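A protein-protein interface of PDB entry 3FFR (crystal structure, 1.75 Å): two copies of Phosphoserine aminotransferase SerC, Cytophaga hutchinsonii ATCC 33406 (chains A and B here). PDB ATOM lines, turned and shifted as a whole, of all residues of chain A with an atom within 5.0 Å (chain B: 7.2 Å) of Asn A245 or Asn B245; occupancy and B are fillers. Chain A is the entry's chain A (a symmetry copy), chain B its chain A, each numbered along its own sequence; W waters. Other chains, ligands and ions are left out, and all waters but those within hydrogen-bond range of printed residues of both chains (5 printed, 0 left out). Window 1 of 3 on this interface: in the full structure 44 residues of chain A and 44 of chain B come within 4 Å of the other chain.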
ATOM      1  N   ALA A 197     -25.762 -10.165   9.610  1.00  0.00           N
ATOM      2  CA  ALA A 197     -24.969 -10.561   8.443  1.00  0.00           C
ATOM      3  C   ALA A 197     -24.313 -11.940   8.712  1.00  0.00           C
ATOM      4  O   ALA A 197     -24.076 -12.338   9.857  1.00  0.00           O
ATOM      5  CB  ALA A 197     -23.915  -9.485   8.079  1.00  0.00           C
ATOM      6  N   GLY A 198     -24.011 -12.607   7.597  1.00  0.00           N
ATOM      7  CA  GLY A 198     -23.372 -13.915   7.568  1.00  0.00           C
ATOM      8  C   GLY A 198     -24.007 -14.949   6.664  1.00  0.00           C
ATOM      9  O   GLY A 198     -23.726 -16.141   6.779  1.00  0.00           O
ATOM     10  N   LEU A 199     -24.789 -14.506   5.679  1.00  0.00           N
ATOM     11  CA  LEU A 199     -25.381 -15.439   4.710  1.00  0.00           C
ATOM     12  C   LEU A 199     -25.782 -14.754   3.409  1.00  0.00           C
ATOM     13  O   LEU A 199     -26.525 -13.775   3.414  1.00  0.00           O
ATOM     14  CB  LEU A 199     -26.625 -16.164   5.319  1.00  0.00           C
ATOM     15  CG  LEU A 199     -27.171 -17.383   4.531  1.00  0.00           C
ATOM     16  CD1 LEU A 199     -26.141 -18.581   4.579  1.00  0.00           C
ATOM     17  CD2 LEU A 199     -28.593 -17.768   5.014  1.00  0.00           C
ATOM     18  N   THR A 243     -19.065 -26.499   6.175  1.00  0.00           N
ATOM     19  CA  THR A 243     -19.956 -26.285   7.323  1.00  0.00           C
ATOM     20  C   THR A 243     -20.501 -24.853   7.190  1.00  0.00           C
ATOM     21  O   THR A 243     -19.727 -23.895   7.201  1.00  0.00           O
ATOM     22  CB  THR A 243     -19.271 -26.483   8.673  1.00  0.00           C
ATOM     23  OG1 THR A 243     -18.472 -27.690   8.622  1.00  0.00           O
ATOM     24  CG2 THR A 243     -20.330 -26.549   9.818  1.00  0.00           C
ATOM     25  N   PRO A 244     -21.823 -24.710   7.085  1.00  0.00           N
ATOM     26  CA  PRO A 244     -22.345 -23.380   6.835  1.00  0.00           C
ATOM     27  C   PRO A 244     -22.801 -22.637   8.071  1.00  0.00           C
ATOM     28  O   PRO A 244     -22.761 -23.168   9.171  1.00  0.00           O
ATOM     29  CB  PRO A 244     -23.581 -23.690   6.031  1.00  0.00           C
ATOM     30  CG  PRO A 244     -24.107 -24.921   6.648  1.00  0.00           C
ATOM     31  CD  PRO A 244     -22.906 -25.728   7.069  1.00  0.00           C
ATOM     32  N   ASN A 245     -23.364 -21.463   7.828  1.00  0.00           N
ATOM     33  CA  ASN A 245     -23.928 -20.634   8.905  1.00  0.00           C
ATOM     34  C   ASN A 245     -25.341 -21.118   9.194  1.00  0.00           C
ATOM     35  O   ASN A 245     -26.333 -20.556   8.742  1.00  0.00           O
ATOM     36  CB  ASN A 245     -23.925 -19.170   8.523  1.00  0.00           C
ATOM     37  CG  ASN A 245     -24.336 -18.277   9.671  1.00  0.00           C
ATOM     38  OD1 ASN A 245     -24.847 -18.756  10.701  1.00  0.00           O
ATOM     39  ND2 ASN A 245     -24.148 -16.955   9.493  1.00  0.00           N
ATOM     40  N   ALA A 246     -25.409 -22.212   9.936  1.00  0.00           N
ATOM     41  CA  ALA A 246     -26.689 -22.826  10.305  1.00  0.00           C
ATOM     42  C   ALA A 246     -27.609 -21.899  11.069  1.00  0.00           C
ATOM     43  O   ALA A 246     -28.836 -21.959  10.946  1.00  0.00           O
ATOM     44  CB  ALA A 246     -26.439 -24.144  11.106  1.00  0.00           C
ATOM     45  N   MET A 247     -27.011 -21.039  11.891  1.00  0.00           N
ATOM     46  CA  MET A 247     -27.814 -20.111  12.697  1.00  0.00           C
ATOM     47  C   MET A 247     -28.644 -19.256  11.758  1.00  0.00           C
ATOM     48  O   MET A 247     -29.882 -19.091  11.925  1.00  0.00           O
ATOM     49  CB  MET A 247     -26.980 -19.233  13.647  1.00  0.00           C
ATOM     50  CG  MET A 247     -26.090 -20.035  14.594  1.00  0.00           C
ATOM     51  SD  MET A 247     -27.104 -21.172  15.822  1.00  0.00           S
ATOM     52  CE  MET A 247     -27.531 -19.951  17.179  1.00  0.00           C
ATOM     53  N   ASN A 248     -27.979 -18.689  10.743  1.00  0.00           N
ATOM     54  CA  ASN A 248     -28.690 -17.844   9.790  1.00  0.00           C
ATOM     55  C   ASN A 248     -29.628 -18.614   8.872  1.00  0.00           C
ATOM     56  O   ASN A 248     -30.656 -18.095   8.464  1.00  0.00           O
ATOM     57  CB  ASN A 248     -27.797 -16.909   8.968  1.00  0.00           C
ATOM     58  CG  ASN A 248     -27.646 -15.547   9.598  1.00  0.00           C
ATOM     59  OD1 ASN A 248     -28.229 -15.250  10.649  1.00  0.00           O
ATOM     60  ND2 ASN A 248     -26.835 -14.684   8.948  1.00  0.00           N
ATOM     61  N   ILE A 249     -29.257 -19.831   8.497  1.00  0.00           N
ATOM     62  CA  ILE A 249     -30.173 -20.647   7.664  1.00  0.00           C
ATOM     63  C   ILE A 249     -31.448 -20.909   8.484  1.00  0.00           C
ATOM     64  O   ILE A 249     -32.574 -20.850   7.982  1.00  0.00           O
ATOM     65  CB  ILE A 249     -29.496 -21.950   7.165  1.00  0.00           C
ATOM     66  CG1 ILE A 249     -28.374 -21.572   6.170  1.00  0.00           C
ATOM     67  CG2 ILE A 249     -30.526 -22.862   6.464  1.00  0.00           C
ATOM     68  CD1 ILE A 249     -27.446 -22.757   5.745  1.00  0.00           C
ATOM     69  N   PHE B  41     -18.253  -1.585  15.840  1.00  0.00           N
ATOM     70  CA  PHE B  41     -17.820  -2.845  15.207  1.00  0.00           C
ATOM     71  C   PHE B  41     -16.301  -2.991  15.253  1.00  0.00           C
ATOM     72  O   PHE B  41     -15.757  -4.086  15.505  1.00  0.00           O
ATOM     73  CB  PHE B  41     -18.322  -3.030  13.744  1.00  0.00           C
ATOM     74  CG  PHE B  41     -17.785  -4.280  13.135  1.00  0.00           C
ATOM     75  CD1 PHE B  41     -18.381  -5.482  13.396  1.00  0.00           C
ATOM     76  CD2 PHE B  41     -16.596  -4.261  12.430  1.00  0.00           C
ATOM     77  CE1 PHE B  41     -17.827  -6.682  12.911  1.00  0.00           C
ATOM     78  CE2 PHE B  41     -16.052  -5.431  11.914  1.00  0.00           C
ATOM     79  CZ  PHE B  41     -16.674  -6.637  12.160  1.00  0.00           C
ATOM     80  N   LEU B  67     -12.449 -14.949   7.735  1.00  0.00           N
ATOM     81  CA  LEU B  67     -13.117 -15.467   6.527  1.00  0.00           C
ATOM     82  C   LEU B  67     -14.378 -16.250   6.916  1.00  0.00           C
ATOM     83  O   LEU B  67     -14.782 -16.269   8.089  1.00  0.00           O
ATOM     84  CB  LEU B  67     -12.186 -16.283   5.636  1.00  0.00           C
ATOM     85  CG  LEU B  67     -10.922 -15.539   5.160  1.00  0.00           C
ATOM     86  CD1 LEU B  67      -9.812 -15.490   6.205  1.00  0.00           C
ATOM     87  CD2 LEU B  67     -10.385 -16.151   3.815  1.00  0.00           C
ATOM     88  N   ALA B  68     -14.993 -16.927   5.948  1.00  0.00           N
ATOM     89  CA  ALA B  68     -16.318 -17.547   6.214  1.00  0.00           C
ATOM     90  C   ALA B  68     -16.230 -18.946   6.774  1.00  0.00           C
ATOM     91  O   ALA B  68     -17.119 -19.413   7.476  1.00  0.00           O
ATOM     92  CB  ALA B  68     -17.155 -17.575   4.910  1.00  0.00           C
ATOM     93  N   VAL B 189     -14.488 -21.920  13.663  1.00  0.00           N
ATOM     94  CA  VAL B 189     -14.874 -21.741  15.074  1.00  0.00           C
ATOM     95  C   VAL B 189     -15.777 -22.775  15.739  1.00  0.00           C
ATOM     96  O   VAL B 189     -15.990 -22.705  16.967  1.00  0.00           O
ATOM     97  CB  VAL B 189     -15.496 -20.335  15.309  1.00  0.00           C
ATOM     98  CG1 VAL B 189     -14.457 -19.213  14.973  1.00  0.00           C
ATOM     99  CG2 VAL B 189     -16.844 -20.151  14.525  1.00  0.00           C
ATOM    100  N   PRO B 196     -21.163 -21.512  17.148  1.00  0.00           N
ATOM    101  CA  PRO B 196     -21.842 -22.019  15.969  1.00  0.00           C
ATOM    102  C   PRO B 196     -20.952 -21.814  14.742  1.00  0.00           C
ATOM    103  O   PRO B 196     -20.147 -20.918  14.710  1.00  0.00           O
ATOM    104  CB  PRO B 196     -23.058 -21.104  15.839  1.00  0.00           C
ATOM    105  CG  PRO B 196     -23.316 -20.631  17.211  1.00  0.00           C
ATOM    106  CD  PRO B 196     -21.904 -20.391  17.753  1.00  0.00           C
ATOM    107  N   ALA B 197     -21.104 -22.662  13.737  1.00  0.00           N
ATOM    108  CA  ALA B 197     -20.336 -22.477  12.502  1.00  0.00           C
ATOM    109  C   ALA B 197     -20.739 -21.132  11.843  1.00  0.00           C
ATOM    110  O   ALA B 197     -21.846 -20.617  12.035  1.00  0.00           O
ATOM    111  CB  ALA B 197     -20.525 -23.671  11.532  1.00  0.00           C
ATOM    112  N   GLY B 198     -19.797 -20.635  11.042  1.00  0.00           N
ATOM    113  CA  GLY B 198     -19.927 -19.395  10.287  1.00  0.00           C
ATOM    114  C   GLY B 198     -18.763 -18.433  10.377  1.00  0.00           C
ATOM    115  O   GLY B 198     -18.887 -17.262  10.021  1.00  0.00           O
ATOM    116  N   LEU B 199     -17.583 -18.931  10.750  1.00  0.00           N
ATOM    117  CA  LEU B 199     -16.385 -18.080  10.786  1.00  0.00           C
ATOM    118  C   LEU B 199     -15.094 -18.885  10.716  1.00  0.00           C
ATOM    119  O   LEU B 199     -14.872 -19.793  11.513  1.00  0.00           O
ATOM    120  CB  LEU B 199     -16.371 -17.188  12.069  1.00  0.00           C
ATOM    121  CG  LEU B 199     -15.333 -16.035  12.101  1.00  0.00           C
ATOM    122  CD1 LEU B 199     -15.703 -14.926  11.037  1.00  0.00           C
ATOM    123  CD2 LEU B 199     -15.159 -15.481  13.539  1.00  0.00           C
ATOM    124  N   THR B 240     -13.395  -5.767   7.727  1.00  0.00           N
ATOM    125  CA  THR B 240     -13.358  -6.802   6.665  1.00  0.00           C
ATOM    126  C   THR B 240     -13.793  -6.184   5.358  1.00  0.00           C
ATOM    127  O   THR B 240     -14.475  -5.173   5.343  1.00  0.00           O
ATOM    128  CB  THR B 240     -14.264  -7.988   7.009  1.00  0.00           C
ATOM    129  OG1 THR B 240     -15.594  -7.526   7.248  1.00  0.00           O
ATOM    130  CG2 THR B 240     -13.744  -8.721   8.303  1.00  0.00           C
ATOM    131  N   GLU B 242     -15.936  -7.304   3.002  1.00  0.00           N
ATOM    132  CA  GLU B 242     -17.381  -7.505   2.869  1.00  0.00           C
ATOM    133  C   GLU B 242     -18.077  -7.426   4.236  1.00  0.00           C
ATOM    134  O   GLU B 242     -17.404  -7.331   5.259  1.00  0.00           O
ATOM    135  CB  GLU B 242     -17.663  -8.863   2.222  1.00  0.00           C
ATOM    136  CG  GLU B 242     -17.650 -10.066   3.181  1.00  0.00           C
ATOM    137  CD  GLU B 242     -16.265 -10.558   3.675  1.00  0.00           C
ATOM    138  OE1 GLU B 242     -15.230  -9.877   3.529  1.00  0.00           O
ATOM    139  OE2 GLU B 242     -16.213 -11.668   4.233  1.00  0.00           O
ATOM    140  N   THR B 243     -19.419  -7.465   4.267  1.00  0.00           N
ATOM    141  CA  THR B 243     -20.114  -7.463   5.561  1.00  0.00           C
ATOM    142  C   THR B 243     -19.885  -8.853   6.180  1.00  0.00           C
ATOM    143  O   THR B 243     -20.288  -9.861   5.600  1.00  0.00           O
ATOM    144  CB  THR B 243     -21.607  -7.156   5.453  1.00  0.00           C
ATOM    145  OG1 THR B 243     -21.790  -6.033   4.557  1.00  0.00           O
ATOM    146  CG2 THR B 243     -22.207  -6.865   6.864  1.00  0.00           C
ATOM    147  N   PRO B 244     -19.259  -8.901   7.356  1.00  0.00           N
ATOM    148  CA  PRO B 244     -18.925 -10.207   7.896  1.00  0.00           C
ATOM    149  C   PRO B 244     -19.920 -10.752   8.894  1.00  0.00           C
ATOM    150  O   PRO B 244     -20.893 -10.095   9.231  1.00  0.00           O
ATOM    151  CB  PRO B 244     -17.662  -9.899   8.660  1.00  0.00           C
ATOM    152  CG  PRO B 244     -17.909  -8.564   9.232  1.00  0.00           C
ATOM    153  CD  PRO B 244     -18.719  -7.809   8.209  1.00  0.00           C
ATOM    154  N   ASN B 245     -19.563 -11.898   9.454  1.00  0.00           N
ATOM    155  CA  ASN B 245     -20.376 -12.540  10.499  1.00  0.00           C
ATOM    156  C   ASN B 245     -20.021 -11.912  11.838  1.00  0.00           C
ATOM    157  O   ASN B 245     -19.249 -12.445  12.628  1.00  0.00           O
ATOM    158  CB  ASN B 245     -20.148 -14.035  10.524  1.00  0.00           C
ATOM    159  CG  ASN B 245     -21.094 -14.745  11.465  1.00  0.00           C
ATOM    160  OD1 ASN B 245     -21.783 -14.104  12.281  1.00  0.00           O
ATOM    161  ND2 ASN B 245     -21.115 -16.089  11.386  1.00  0.00           N
ATOM    162  N   ALA B 246     -20.580 -10.733  12.061  1.00  0.00           N
ATOM    163  CA  ALA B 246     -20.342  -9.978  13.296  1.00  0.00           C
ATOM    164  C   ALA B 246     -20.733 -10.728  14.550  1.00  0.00           C
ATOM    165  O   ALA B 246     -20.114 -10.585  15.609  1.00  0.00           O
ATOM    166  CB  ALA B 246     -21.067  -8.596  13.225  1.00  0.00           C
ATOM    167  N   MET B 247     -21.794 -11.524  14.441  1.00  0.00           N
ATOM    168  CA  MET B 247     -22.271 -12.279  15.607  1.00  0.00           C
ATOM    169  C   MET B 247     -21.147 -13.173  16.092  1.00  0.00           C
ATOM    170  O   MET B 247     -20.804 -13.217  17.303  1.00  0.00           O
ATOM    171  CB  MET B 247     -23.547 -13.097  15.336  1.00  0.00           C
ATOM    172  CG  MET B 247     -24.707 -12.258  14.806  1.00  0.00           C
ATOM    173  SD  MET B 247     -25.318 -10.900  16.077  1.00  0.00           S
ATOM    174  CE  MET B 247     -26.473 -11.907  17.157  1.00  0.00           C
ATOM    175  N   ASN B 248     -20.543 -13.913  15.152  1.00  0.00           N
ATOM    176  CA  ASN B 248     -19.453 -14.810  15.523  1.00  0.00           C
ATOM    177  C   ASN B 248     -18.173 -14.086  15.914  1.00  0.00           C
ATOM    178  O   ASN B 248     -17.422 -14.566  16.749  1.00  0.00           O
ATOM    179  CB  ASN B 248     -19.146 -15.908  14.499  1.00  0.00           C
ATOM    180  CG  ASN B 248     -19.890 -17.189  14.780  1.00  0.00           C
ATOM    181  OD1 ASN B 248     -20.630 -17.307  15.766  1.00  0.00           O
ATOM    182  ND2 ASN B 248     -19.701 -18.188  13.891  1.00  0.00           N
ATOM    183  N   ILE B 249     -17.887 -12.959  15.277  1.00  0.00           N
ATOM    184  CA  ILE B 249     -16.689 -12.181  15.676  1.00  0.00           C
ATOM    185  C   ILE B 249     -16.890 -11.718  17.130  1.00  0.00           C
ATOM    186  O   ILE B 249     -15.978 -11.748  17.960  1.00  0.00           O
ATOM    187  CB  ILE B 249     -16.408 -11.007  14.701  1.00  0.00           C
ATOM    188  CG1 ILE B 249     -15.994 -11.594  13.332  1.00  0.00           C
ATOM    189  CG2 ILE B 249     -15.277 -10.109  15.245  1.00  0.00           C
ATOM    190  CD1 ILE B 249     -15.894 -10.548  12.173  1.00  0.00           C
ATOM    191  N   PHE B 250     -18.123 -11.323  17.436  1.00  0.00           N
ATOM    192  CA  PHE B 250     -18.480 -10.900  18.798  1.00  0.00           C
ATOM    193  C   PHE B 250     -18.316 -12.055  19.777  1.00  0.00           C
ATOM    194  O   PHE B 250     -17.647 -11.959  20.822  1.00  0.00           O
ATOM    195  CB  PHE B 250     -19.930 -10.412  18.851  1.00  0.00           C
ATOM    196  CG  PHE B 250     -20.383  -9.981  20.215  1.00  0.00           C
ATOM    197  CD1 PHE B 250     -20.085  -8.700  20.681  1.00  0.00           C
ATOM    198  CD2 PHE B 250     -21.144 -10.814  21.007  1.00  0.00           C
ATOM    199  CE1 PHE B 250     -20.523  -8.276  21.921  1.00  0.00           C
ATOM    200  CE2 PHE B 250     -21.578 -10.392  22.256  1.00  0.00           C
ATOM    201  CZ  PHE B 250     -21.259  -9.121  22.705  1.00  0.00           C
ATOM    202  N   LEU B 251     -18.927 -13.175  19.428  1.00  0.00           N
ATOM    203  CA  LEU B 251     -18.887 -14.339  20.308  1.00  0.00           C
ATOM    204  C   LEU B 251     -17.455 -14.829  20.481  1.00  0.00           C
ATOM    205  O   LEU B 251     -17.061 -15.260  21.566  1.00  0.00           O
ATOM    206  CB  LEU B 251     -19.769 -15.479  19.779  1.00  0.00           C
ATOM    207  CG  LEU B 251     -21.282 -15.272  19.767  1.00  0.00           C
ATOM    208  CD1 LEU B 251     -21.911 -16.493  19.070  1.00  0.00           C
ATOM    209  CD2 LEU B 251     -21.855 -15.058  21.210  1.00  0.00           C
HETATM  210  O   HOH W   1     -24.398 -14.635  11.495  1.00  0.00           O
HETATM  211  O   HOH W   2     -23.607 -10.643  11.991  1.00  0.00           O
HETATM  212  O   HOH W   3     -19.434 -21.034   7.393  1.00  0.00           O
HETATM  213  O   HOH W   4     -23.018 -18.117  12.698  1.00  0.00           O
HETATM  214  O   HOH W   5     -24.112 -22.067  12.669  1.00  0.00           O
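The backbone carbonyl oxygen (O) of Pro B196 sits at hydrogen-bond distance from the side-chain amide nitrogen (ND2) of Asn B248, at 2.9 Å. The side-chain amide nitrogen of Asn B245 sits at hydrogen-bond distance from the backbone carbonyl oxygen of Gly B198, 2.9 Å away. N of Met B247 sits close to OD1 of Asn B245, at 3.4 Å. OD1 of Asn B245 lies within hydrogen-bond range of N of Asn B248. OD1 of Asn A245 lies close to N of Met A247. The side-chain amide oxygen (OD1) of Asn A245 is in hydrogen-bond range of the backbone NH (N) of Asn A248, at 3.1 Å.
Ala A197 touches Thr B243. O of Pro B244 touches CB of Ala A197 (3.3 Å). O of Ala A197 touches CA of Asn B245, 3.8 Å away. Thr A243 touches Ala B197 (CG2 to CB, 3.4 Å). Ala B197 touches Pro A244 (CB to O, 3.3 Å). Ala B197 touches Asn A245 (O to CA, 3.8 Å). Asn B245 touches Asn A245 (ND2 to ND2, 3.7 Å). Pro B196 touches Met A247.
Asn A245 touches two residues of chain B. Of the printed residues of chain A, Pro B196 touches Met A247. Of the printed residues of chain B, Ala A197 touches Thr B243 (3.4 Å), Pro B244 (3.3 Å) and Asn B245 (3.8 Å). Leu A199 touches none of the printed residues of chain B. The nearest printed residue of chain A that does not touch Ala B197 is Ala A246 (4.4 Å).
Of the 10 printed residues of chain A, 5 touch a printed residue of chain B. Printed residues of chain A that touch a printed residue of chain B: Ala A197, Thr A243, Pro A244, Asn A245 and Met A247. Hydrophobic or aromatic side chains of chain A that line the printed part of chain B: Ala A197 and Met A247. Of the 19 printed residues of chain B, 5 touch a printed residue of chain A. Printed residues of chain B that touch a printed residue of chain A: Pro B196, Ala B197, Thr B243, Pro B244 and Asn B245. Hydrophobic or aromatic side chains of chain B that line the printed part of chain A: Pro B196 and Ala B197.
Ala A197 touches Thr B243, and with the chains exchanged Thr A243 touches Ala B197. Ala A197 touches Pro B244, and with the chains exchanged Pro A244 touches Ala B197. Ala A197 touches Asn B245, and with the chains exchanged Asn A245 touches Ala B197. Asn B245 touches its own counterpart, Asn A245. Positions printed for both chains: 197, 198, 199, 243, 244, 245, 246, 247, 248 and 249.
Water W5 lies within hydrogen-bond range of O of Ala B197 (2.8 Å), N of Ala A246 (3.0 Å) and N of Met A247 (3.2 Å). Water W2 lies within hydrogen-bond range of the backbone carbonyl oxygen (O) of Ala A197, the backbone NH (N) of Ala B246 and the backbone NH (N) of Met B247. Water W1 lies within hydrogen-bond range of OD1 of Asn B245, O of Ala A197 and ND2 of Asn A245. Water W4 lies within hydrogen-bond range of OD1 of Asn A245 (2.8 Å), O of Ala B197 (2.8 Å) and ND2 of Asn B245 (3.1 Å). Water W3 lies within hydrogen-bond range of O of Ala B68 (2.8 Å) and O of Thr A243 (2.9 Å).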
